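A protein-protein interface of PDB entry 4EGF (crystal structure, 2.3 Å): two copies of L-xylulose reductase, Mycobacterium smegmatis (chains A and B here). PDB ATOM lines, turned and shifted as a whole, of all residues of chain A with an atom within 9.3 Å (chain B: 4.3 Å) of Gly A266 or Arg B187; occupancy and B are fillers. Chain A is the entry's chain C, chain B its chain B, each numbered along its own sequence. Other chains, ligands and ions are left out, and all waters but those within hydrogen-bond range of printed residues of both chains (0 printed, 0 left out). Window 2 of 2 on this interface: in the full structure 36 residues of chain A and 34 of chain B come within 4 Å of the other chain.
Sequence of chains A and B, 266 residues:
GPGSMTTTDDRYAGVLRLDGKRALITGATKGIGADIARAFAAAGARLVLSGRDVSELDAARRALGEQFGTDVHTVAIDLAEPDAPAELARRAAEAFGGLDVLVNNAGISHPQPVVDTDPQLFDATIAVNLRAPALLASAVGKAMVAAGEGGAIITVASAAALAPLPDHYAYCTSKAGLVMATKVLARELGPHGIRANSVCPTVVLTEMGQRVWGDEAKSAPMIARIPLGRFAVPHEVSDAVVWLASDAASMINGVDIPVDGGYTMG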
ATOM      1  N   LEU A 162      24.067  29.897 -16.330  1.00  0.00           N
ATOM      2  CA  LEU A 162      23.058  29.028 -15.681  1.00  0.00           C
ATOM      3  C   LEU A 162      23.601  27.713 -15.182  1.00  0.00           C
ATOM      4  O   LEU A 162      22.944  27.046 -14.392  1.00  0.00           O
ATOM      5  CB  LEU A 162      21.909  28.725 -16.648  1.00  0.00           C
ATOM      6  CG  LEU A 162      21.394  29.939 -17.404  1.00  0.00           C
ATOM      7  CD1 LEU A 162      20.398  29.482 -18.433  1.00  0.00           C
ATOM      8  CD2 LEU A 162      20.827  31.009 -16.434  1.00  0.00           C
ATOM      9  N   ALA A 163      24.775  27.306 -15.637  1.00  0.00           N
ATOM     10  CA  ALA A 163      25.338  26.033 -15.192  1.00  0.00           C
ATOM     11  C   ALA A 163      26.854  26.129 -15.265  1.00  0.00           C
ATOM     12  O   ALA A 163      27.388  26.668 -16.211  1.00  0.00           O
ATOM     13  CB  ALA A 163      24.833  24.900 -16.071  1.00  0.00           C
ATOM     14  N   PRO A 164      27.546  25.615 -14.251  1.00  0.00           N
ATOM     15  CA  PRO A 164      28.948  25.832 -14.157  1.00  0.00           C
ATOM     16  C   PRO A 164      29.676  25.027 -15.226  1.00  0.00           C
ATOM     17  O   PRO A 164      29.269  23.937 -15.538  1.00  0.00           O
ATOM     18  CB  PRO A 164      29.278  25.343 -12.738  1.00  0.00           C
ATOM     19  CG  PRO A 164      28.306  24.265 -12.492  1.00  0.00           C
ATOM     20  CD  PRO A 164      27.061  24.678 -13.217  1.00  0.00           C
ATOM     21  N   ILE A 223      28.701  18.474 -26.873  1.00  0.00           N
ATOM     22  CA  ILE A 223      27.567  18.172 -27.720  1.00  0.00           C
ATOM     23  C   ILE A 223      26.728  17.020 -27.146  1.00  0.00           C
ATOM     24  O   ILE A 223      25.477  17.075 -27.132  1.00  0.00           O
ATOM     25  CB  ILE A 223      28.016  17.915 -29.155  1.00  0.00           C
ATOM     26  CG1 ILE A 223      28.448  19.262 -29.768  1.00  0.00           C
ATOM     27  CG2 ILE A 223      26.898  17.219 -29.942  1.00  0.00           C
ATOM     28  CD1 ILE A 223      28.409  19.314 -31.279  1.00  0.00           C
ATOM     29  N   ALA A 224      27.415  16.019 -26.613  1.00  0.00           N
ATOM     30  CA  ALA A 224      26.752  14.939 -25.902  1.00  0.00           C
ATOM     31  C   ALA A 224      25.669  15.483 -24.970  1.00  0.00           C
ATOM     32  O   ALA A 224      24.631  14.855 -24.794  1.00  0.00           O
ATOM     33  CB  ALA A 224      27.761  14.102 -25.106  1.00  0.00           C
ATOM     34  N   ARG A 225      25.936  16.642 -24.382  1.00  0.00           N
ATOM     35  CA  ARG A 225      25.065  17.231 -23.380  1.00  0.00           C
ATOM     36  C   ARG A 225      24.002  18.147 -23.962  1.00  0.00           C
ATOM     37  O   ARG A 225      23.218  18.694 -23.198  1.00  0.00           O
ATOM     38  CB  ARG A 225      25.892  18.014 -22.363  1.00  0.00           C
ATOM     39  CG  ARG A 225      26.659  17.122 -21.410  1.00  0.00           C
ATOM     40  CD  ARG A 225      25.868  16.847 -20.169  1.00  0.00           C
ATOM     41  NE  ARG A 225      26.115  17.884 -19.168  1.00  0.00           N
ATOM     42  CZ  ARG A 225      25.271  18.860 -18.813  1.00  0.00           C
ATOM     43  NH1 ARG A 225      24.047  19.010 -19.375  1.00  0.00           N
ATOM     44  NH2 ARG A 225      25.673  19.713 -17.876  1.00  0.00           N
ATOM     45  N   ILE A 226      24.018  18.341 -25.289  1.00  0.00           N
ATOM     46  CA  ILE A 226      22.955  19.063 -26.011  1.00  0.00           C
ATOM     47  C   ILE A 226      22.008  18.077 -26.747  1.00  0.00           C
ATOM     48  O   ILE A 226      22.417  17.371 -27.687  1.00  0.00           O
ATOM     49  CB  ILE A 226      23.485  20.117 -27.012  1.00  0.00           C
ATOM     50  CG1 ILE A 226      24.379  21.129 -26.309  1.00  0.00           C
ATOM     51  CG2 ILE A 226      22.312  20.852 -27.677  1.00  0.00           C
ATOM     52  CD1 ILE A 226      25.258  21.972 -27.247  1.00  0.00           C
ATOM     53  N   PRO A 227      20.733  18.031 -26.307  1.00  0.00           N
ATOM     54  CA  PRO A 227      19.800  17.079 -26.919  1.00  0.00           C
ATOM     55  C   PRO A 227      19.565  17.231 -28.412  1.00  0.00           C
ATOM     56  O   PRO A 227      19.399  16.226 -29.091  1.00  0.00           O
ATOM     57  CB  PRO A 227      18.527  17.303 -26.125  1.00  0.00           C
ATOM     58  CG  PRO A 227      19.038  17.640 -24.752  1.00  0.00           C
ATOM     59  CD  PRO A 227      20.290  18.432 -24.960  1.00  0.00           C
ATOM     60  N   LEU A 228      19.558  18.457 -28.938  1.00  0.00           N
ATOM     61  CA  LEU A 228      19.466  18.651 -30.390  1.00  0.00           C
ATOM     62  C   LEU A 228      20.754  18.273 -31.184  1.00  0.00           C
ATOM     63  O   LEU A 228      20.728  18.231 -32.423  1.00  0.00           O
ATOM     64  CB  LEU A 228      19.079  20.065 -30.706  1.00  0.00           C
ATOM     65  CG  LEU A 228      17.709  20.549 -30.224  1.00  0.00           C
ATOM     66  CD1 LEU A 228      17.527  21.969 -30.750  1.00  0.00           C
ATOM     67  CD2 LEU A 228      16.575  19.647 -30.688  1.00  0.00           C
ATOM     68  N   GLY A 229      21.859  17.999 -30.494  1.00  0.00           N
ATOM     69  CA  GLY A 229      23.089  17.462 -31.159  1.00  0.00           C
ATOM     70  C   GLY A 229      23.992  18.449 -31.926  1.00  0.00           C
ATOM     71  O   GLY A 229      24.813  18.024 -32.718  1.00  0.00           O
ATOM     72  N   ASP A 260      19.920  26.887 -26.300  1.00  0.00           N
ATOM     73  CA  ASP A 260      20.912  25.809 -26.031  1.00  0.00           C
ATOM     74  C   ASP A 260      20.489  24.362 -26.300  1.00  0.00           C
ATOM     75  O   ASP A 260      21.084  23.415 -25.727  1.00  0.00           O
ATOM     76  CB  ASP A 260      21.310  25.907 -24.564  1.00  0.00           C
ATOM     77  CG  ASP A 260      20.184  25.461 -23.591  1.00  0.00           C
ATOM     78  OD1 ASP A 260      19.001  25.225 -24.015  1.00  0.00           O
ATOM     79  OD2 ASP A 260      20.530  25.315 -22.374  1.00  0.00           O
ATOM     80  N   GLY A 261      19.481  24.159 -27.138  1.00  0.00           N
ATOM     81  CA  GLY A 261      19.116  22.797 -27.551  1.00  0.00           C
ATOM     82  C   GLY A 261      18.705  21.837 -26.427  1.00  0.00           C
ATOM     83  O   GLY A 261      18.483  20.622 -26.672  1.00  0.00           O
ATOM     84  N   GLY A 262      18.585  22.380 -25.202  1.00  0.00           N
ATOM     85  CA  GLY A 262      18.238  21.617 -24.014  1.00  0.00           C
ATOM     86  C   GLY A 262      19.341  21.417 -22.967  1.00  0.00           C
ATOM     87  O   GLY A 262      19.117  20.730 -21.951  1.00  0.00           O
ATOM     88  N   TYR A 263      20.515  22.010 -23.184  1.00  0.00           N
ATOM     89  CA  TYR A 263      21.703  21.679 -22.376  1.00  0.00           C
ATOM     90  C   TYR A 263      21.426  21.935 -20.892  1.00  0.00           C
ATOM     91  O   TYR A 263      21.691  21.059 -20.031  1.00  0.00           O
ATOM     92  CB  TYR A 263      22.907  22.502 -22.837  1.00  0.00           C
ATOM     93  CG  TYR A 263      24.199  22.331 -22.063  1.00  0.00           C
ATOM     94  CD1 TYR A 263      24.394  22.932 -20.834  1.00  0.00           C
ATOM     95  CD2 TYR A 263      25.271  21.637 -22.620  1.00  0.00           C
ATOM     96  CE1 TYR A 263      25.605  22.811 -20.155  1.00  0.00           C
ATOM     97  CE2 TYR A 263      26.489  21.512 -21.955  1.00  0.00           C
ATOM     98  CZ  TYR A 263      26.656  22.092 -20.726  1.00  0.00           C
ATOM     99  OH  TYR A 263      27.874  21.947 -20.071  1.00  0.00           O
ATOM    100  N   THR A 264      20.893  23.124 -20.611  1.00  0.00           N
ATOM    101  CA  THR A 264      20.751  23.610 -19.224  1.00  0.00           C
ATOM    102  C   THR A 264      19.594  22.990 -18.435  1.00  0.00           C
ATOM    103  O   THR A 264      19.427  23.333 -17.279  1.00  0.00           O
ATOM    104  CB  THR A 264      20.678  25.166 -19.144  1.00  0.00           C
ATOM    105  OG1 THR A 264      19.452  25.637 -19.729  1.00  0.00           O
ATOM    106  CG2 THR A 264      21.835  25.770 -19.900  1.00  0.00           C
ATOM    107  N   MET A 265      18.813  22.086 -19.039  1.00  0.00           N
ATOM    108  CA  MET A 265      17.874  21.249 -18.246  1.00  0.00           C
ATOM    109  C   MET A 265      18.656  20.367 -17.317  1.00  0.00           C
ATOM    110  O   MET A 265      18.156  19.957 -16.266  1.00  0.00           O
ATOM    111  CB  MET A 265      17.031  20.302 -19.092  1.00  0.00           C
ATOM    112  CG  MET A 265      16.133  20.901 -20.174  1.00  0.00           C
ATOM    113  SD  MET A 265      15.165  19.594 -20.970  1.00  0.00           S
ATOM    114  CE  MET A 265      16.468  18.446 -21.457  1.00  0.00           C
ATOM    115  N   GLY A 266      19.882  20.034 -17.712  1.00  0.00           N
ATOM    116  CA  GLY A 266      20.695  19.134 -16.924  1.00  0.00           C
ATOM    117  C   GLY A 266      20.197  17.707 -17.061  1.00  0.00           C
ATOM    118  O   GLY A 266      19.592  17.357 -18.110  1.00  0.00           O
ATOM    119  OXT GLY A 266      20.418  16.878 -16.134  1.00  0.00           O
ATOM    120  N   LYS B 183      10.139  18.347 -20.173  1.00  0.00           N
ATOM    121  CA  LYS B 183      11.598  18.300 -20.234  1.00  0.00           C
ATOM    122  C   LYS B 183      12.135  16.934 -20.559  1.00  0.00           C
ATOM    123  O   LYS B 183      13.118  16.846 -21.237  1.00  0.00           O
ATOM    124  CB  LYS B 183      12.236  18.812 -18.938  1.00  0.00           C
ATOM    125  CG  LYS B 183      11.854  20.263 -18.670  1.00  0.00           C
ATOM    126  CD  LYS B 183      12.799  20.963 -17.740  1.00  0.00           C
ATOM    127  CE  LYS B 183      12.214  22.331 -17.421  1.00  0.00           C
ATOM    128  NZ  LYS B 183      11.165  22.125 -16.380  1.00  0.00           N
ATOM    129  N   VAL B 184      11.486  15.873 -20.101  1.00  0.00           N
ATOM    130  CA  VAL B 184      11.871  14.517 -20.529  1.00  0.00           C
ATOM    131  C   VAL B 184      11.685  14.314 -22.049  1.00  0.00           C
ATOM    132  O   VAL B 184      12.553  13.739 -22.744  1.00  0.00           O
ATOM    133  CB  VAL B 184      11.066  13.447 -19.764  1.00  0.00           C
ATOM    134  CG1 VAL B 184      11.252  12.049 -20.375  1.00  0.00           C
ATOM    135  CG2 VAL B 184      11.449  13.482 -18.298  1.00  0.00           C
ATOM    136  N   LEU B 185      10.552  14.762 -22.562  1.00  0.00           N
ATOM    137  CA  LEU B 185      10.338  14.793 -24.005  1.00  0.00           C
ATOM    138  C   LEU B 185      11.494  15.533 -24.676  1.00  0.00           C
ATOM    139  O   LEU B 185      12.177  14.959 -25.559  1.00  0.00           O
ATOM    140  CB  LEU B 185       9.007  15.439 -24.347  1.00  0.00           C
ATOM    141  CG  LEU B 185       7.784  14.576 -23.965  1.00  0.00           C
ATOM    142  CD1 LEU B 185       6.530  15.417 -23.807  1.00  0.00           C
ATOM    143  CD2 LEU B 185       7.578  13.436 -24.955  1.00  0.00           C
ATOM    144  N   ALA B 186      11.741  16.772 -24.215  1.00  0.00           N
ATOM    145  CA  ALA B 186      12.849  17.593 -24.738  1.00  0.00           C
ATOM    146  C   ALA B 186      14.155  16.794 -24.798  1.00  0.00           C
ATOM    147  O   ALA B 186      14.857  16.812 -25.811  1.00  0.00           O
ATOM    148  CB  ALA B 186      13.038  18.867 -23.913  1.00  0.00           C
ATOM    149  N   ARG B 187      14.470  16.123 -23.691  1.00  0.00           N
ATOM    150  CA  ARG B 187      15.692  15.329 -23.558  1.00  0.00           C
ATOM    151  C   ARG B 187      15.803  14.116 -24.519  1.00  0.00           C
ATOM    152  O   ARG B 187      16.857  13.880 -25.081  1.00  0.00           O
ATOM    153  CB  ARG B 187      15.780  14.841 -22.124  1.00  0.00           C
ATOM    154  CG  ARG B 187      16.919  13.880 -21.818  1.00  0.00           C
ATOM    155  CD  ARG B 187      18.306  14.458 -22.109  1.00  0.00           C
ATOM    156  NE  ARG B 187      19.353  13.416 -21.979  1.00  0.00           N
ATOM    157  CZ  ARG B 187      20.047  13.164 -20.862  1.00  0.00           C
ATOM    158  NH1 ARG B 187      19.849  13.872 -19.731  1.00  0.00           N
ATOM    159  NH2 ARG B 187      20.959  12.192 -20.868  1.00  0.00           N
ATOM    160  N   GLU B 188      14.727  13.350 -24.676  1.00  0.00           N
ATOM    161  CA  GLU B 188      14.770  12.100 -25.465  1.00  0.00           C
ATOM    162  C   GLU B 188      14.442  12.308 -26.949  1.00  0.00           C
ATOM    163  O   GLU B 188      14.997  11.641 -27.825  1.00  0.00           O
ATOM    164  CB  GLU B 188      13.799  11.065 -24.887  1.00  0.00           C
ATOM    165  CG  GLU B 188      14.157  10.520 -23.512  1.00  0.00           C
ATOM    166  CD  GLU B 188      13.220   9.404 -23.013  1.00  0.00           C
ATOM    167  OE1 GLU B 188      13.138   9.182 -21.773  1.00  0.00           O
ATOM    168  OE2 GLU B 188      12.549   8.753 -23.836  1.00  0.00           O
ATOM    169  N   LEU B 189      13.506  13.217 -27.218  1.00  0.00           N
ATOM    170  CA  LEU B 189      13.033  13.479 -28.573  1.00  0.00           C
ATOM    171  C   LEU B 189      13.874  14.562 -29.281  1.00  0.00           C
ATOM    172  O   LEU B 189      13.893  14.630 -30.524  1.00  0.00           O
ATOM    173  CB  LEU B 189      11.533  13.819 -28.549  1.00  0.00           C
ATOM    174  CG  LEU B 189      10.599  12.791 -27.838  1.00  0.00           C
ATOM    175  CD1 LEU B 189       9.143  13.215 -27.914  1.00  0.00           C
ATOM    176  CD2 LEU B 189      10.734  11.386 -28.388  1.00  0.00           C
ATOM    177  N   PRO B 191      17.128  14.567 -29.886  1.00  0.00           N
ATOM    178  CA  PRO B 191      17.994  13.971 -30.926  1.00  0.00           C
ATOM    179  C   PRO B 191      17.265  13.590 -32.221  1.00  0.00           C
ATOM    180  O   PRO B 191      17.931  13.332 -33.218  1.00  0.00           O
ATOM    181  CB  PRO B 191      18.599  12.733 -30.227  1.00  0.00           C
ATOM    182  CG  PRO B 191      18.533  13.046 -28.778  1.00  0.00           C
ATOM    183  CD  PRO B 191      17.246  13.843 -28.612  1.00  0.00           C
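No position is printed for both chains. Of the 7 pairs that touch across the chains among the printed residues, none has its exchanged pair printed and touching as well.
Pro A227 touches Ala B186 (CB to O, 3.7 Å). CB of Pro A227 touches O of Arg B187, 3.9 Å away. Ala B186 touches Met A265. Met A265 touches Arg B187 (CE to CB, 3.7 Å).
O of Gly A266 is in salt-bridge range of NH1 of Arg B187 (3.9 Å). N of Pro B191 lies close to O of Pro A227, at 2.9 Å. The side-chain sulfur (SD) of Met A265 sits close to the backbone carbonyl oxygen (O) of Lys B183 (3.4 Å).
Of the 17 printed residues of chain A, 3 touch a printed residue of chain B. Printed residues of chain A that touch a printed residue of chain B: Pro A227, Met A265 and Gly A266. Among the printed residues, 7 pairs touch across the chains.
Gly A266 touches just one residue of chain B: Arg B187. Printed residues of chain A within 4 Å of Ala B186: Pro A227 and Met A265. Printed residues of chain B within 4 Å of Met A265: Lys B183, Ala B186 and Arg B187. Printed residues of chain A within 4 Å of Pro B191: Pro A227. The nearest printed residue of chain B that does not touch Pro A227 is Glu B188 (5.7 Å).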
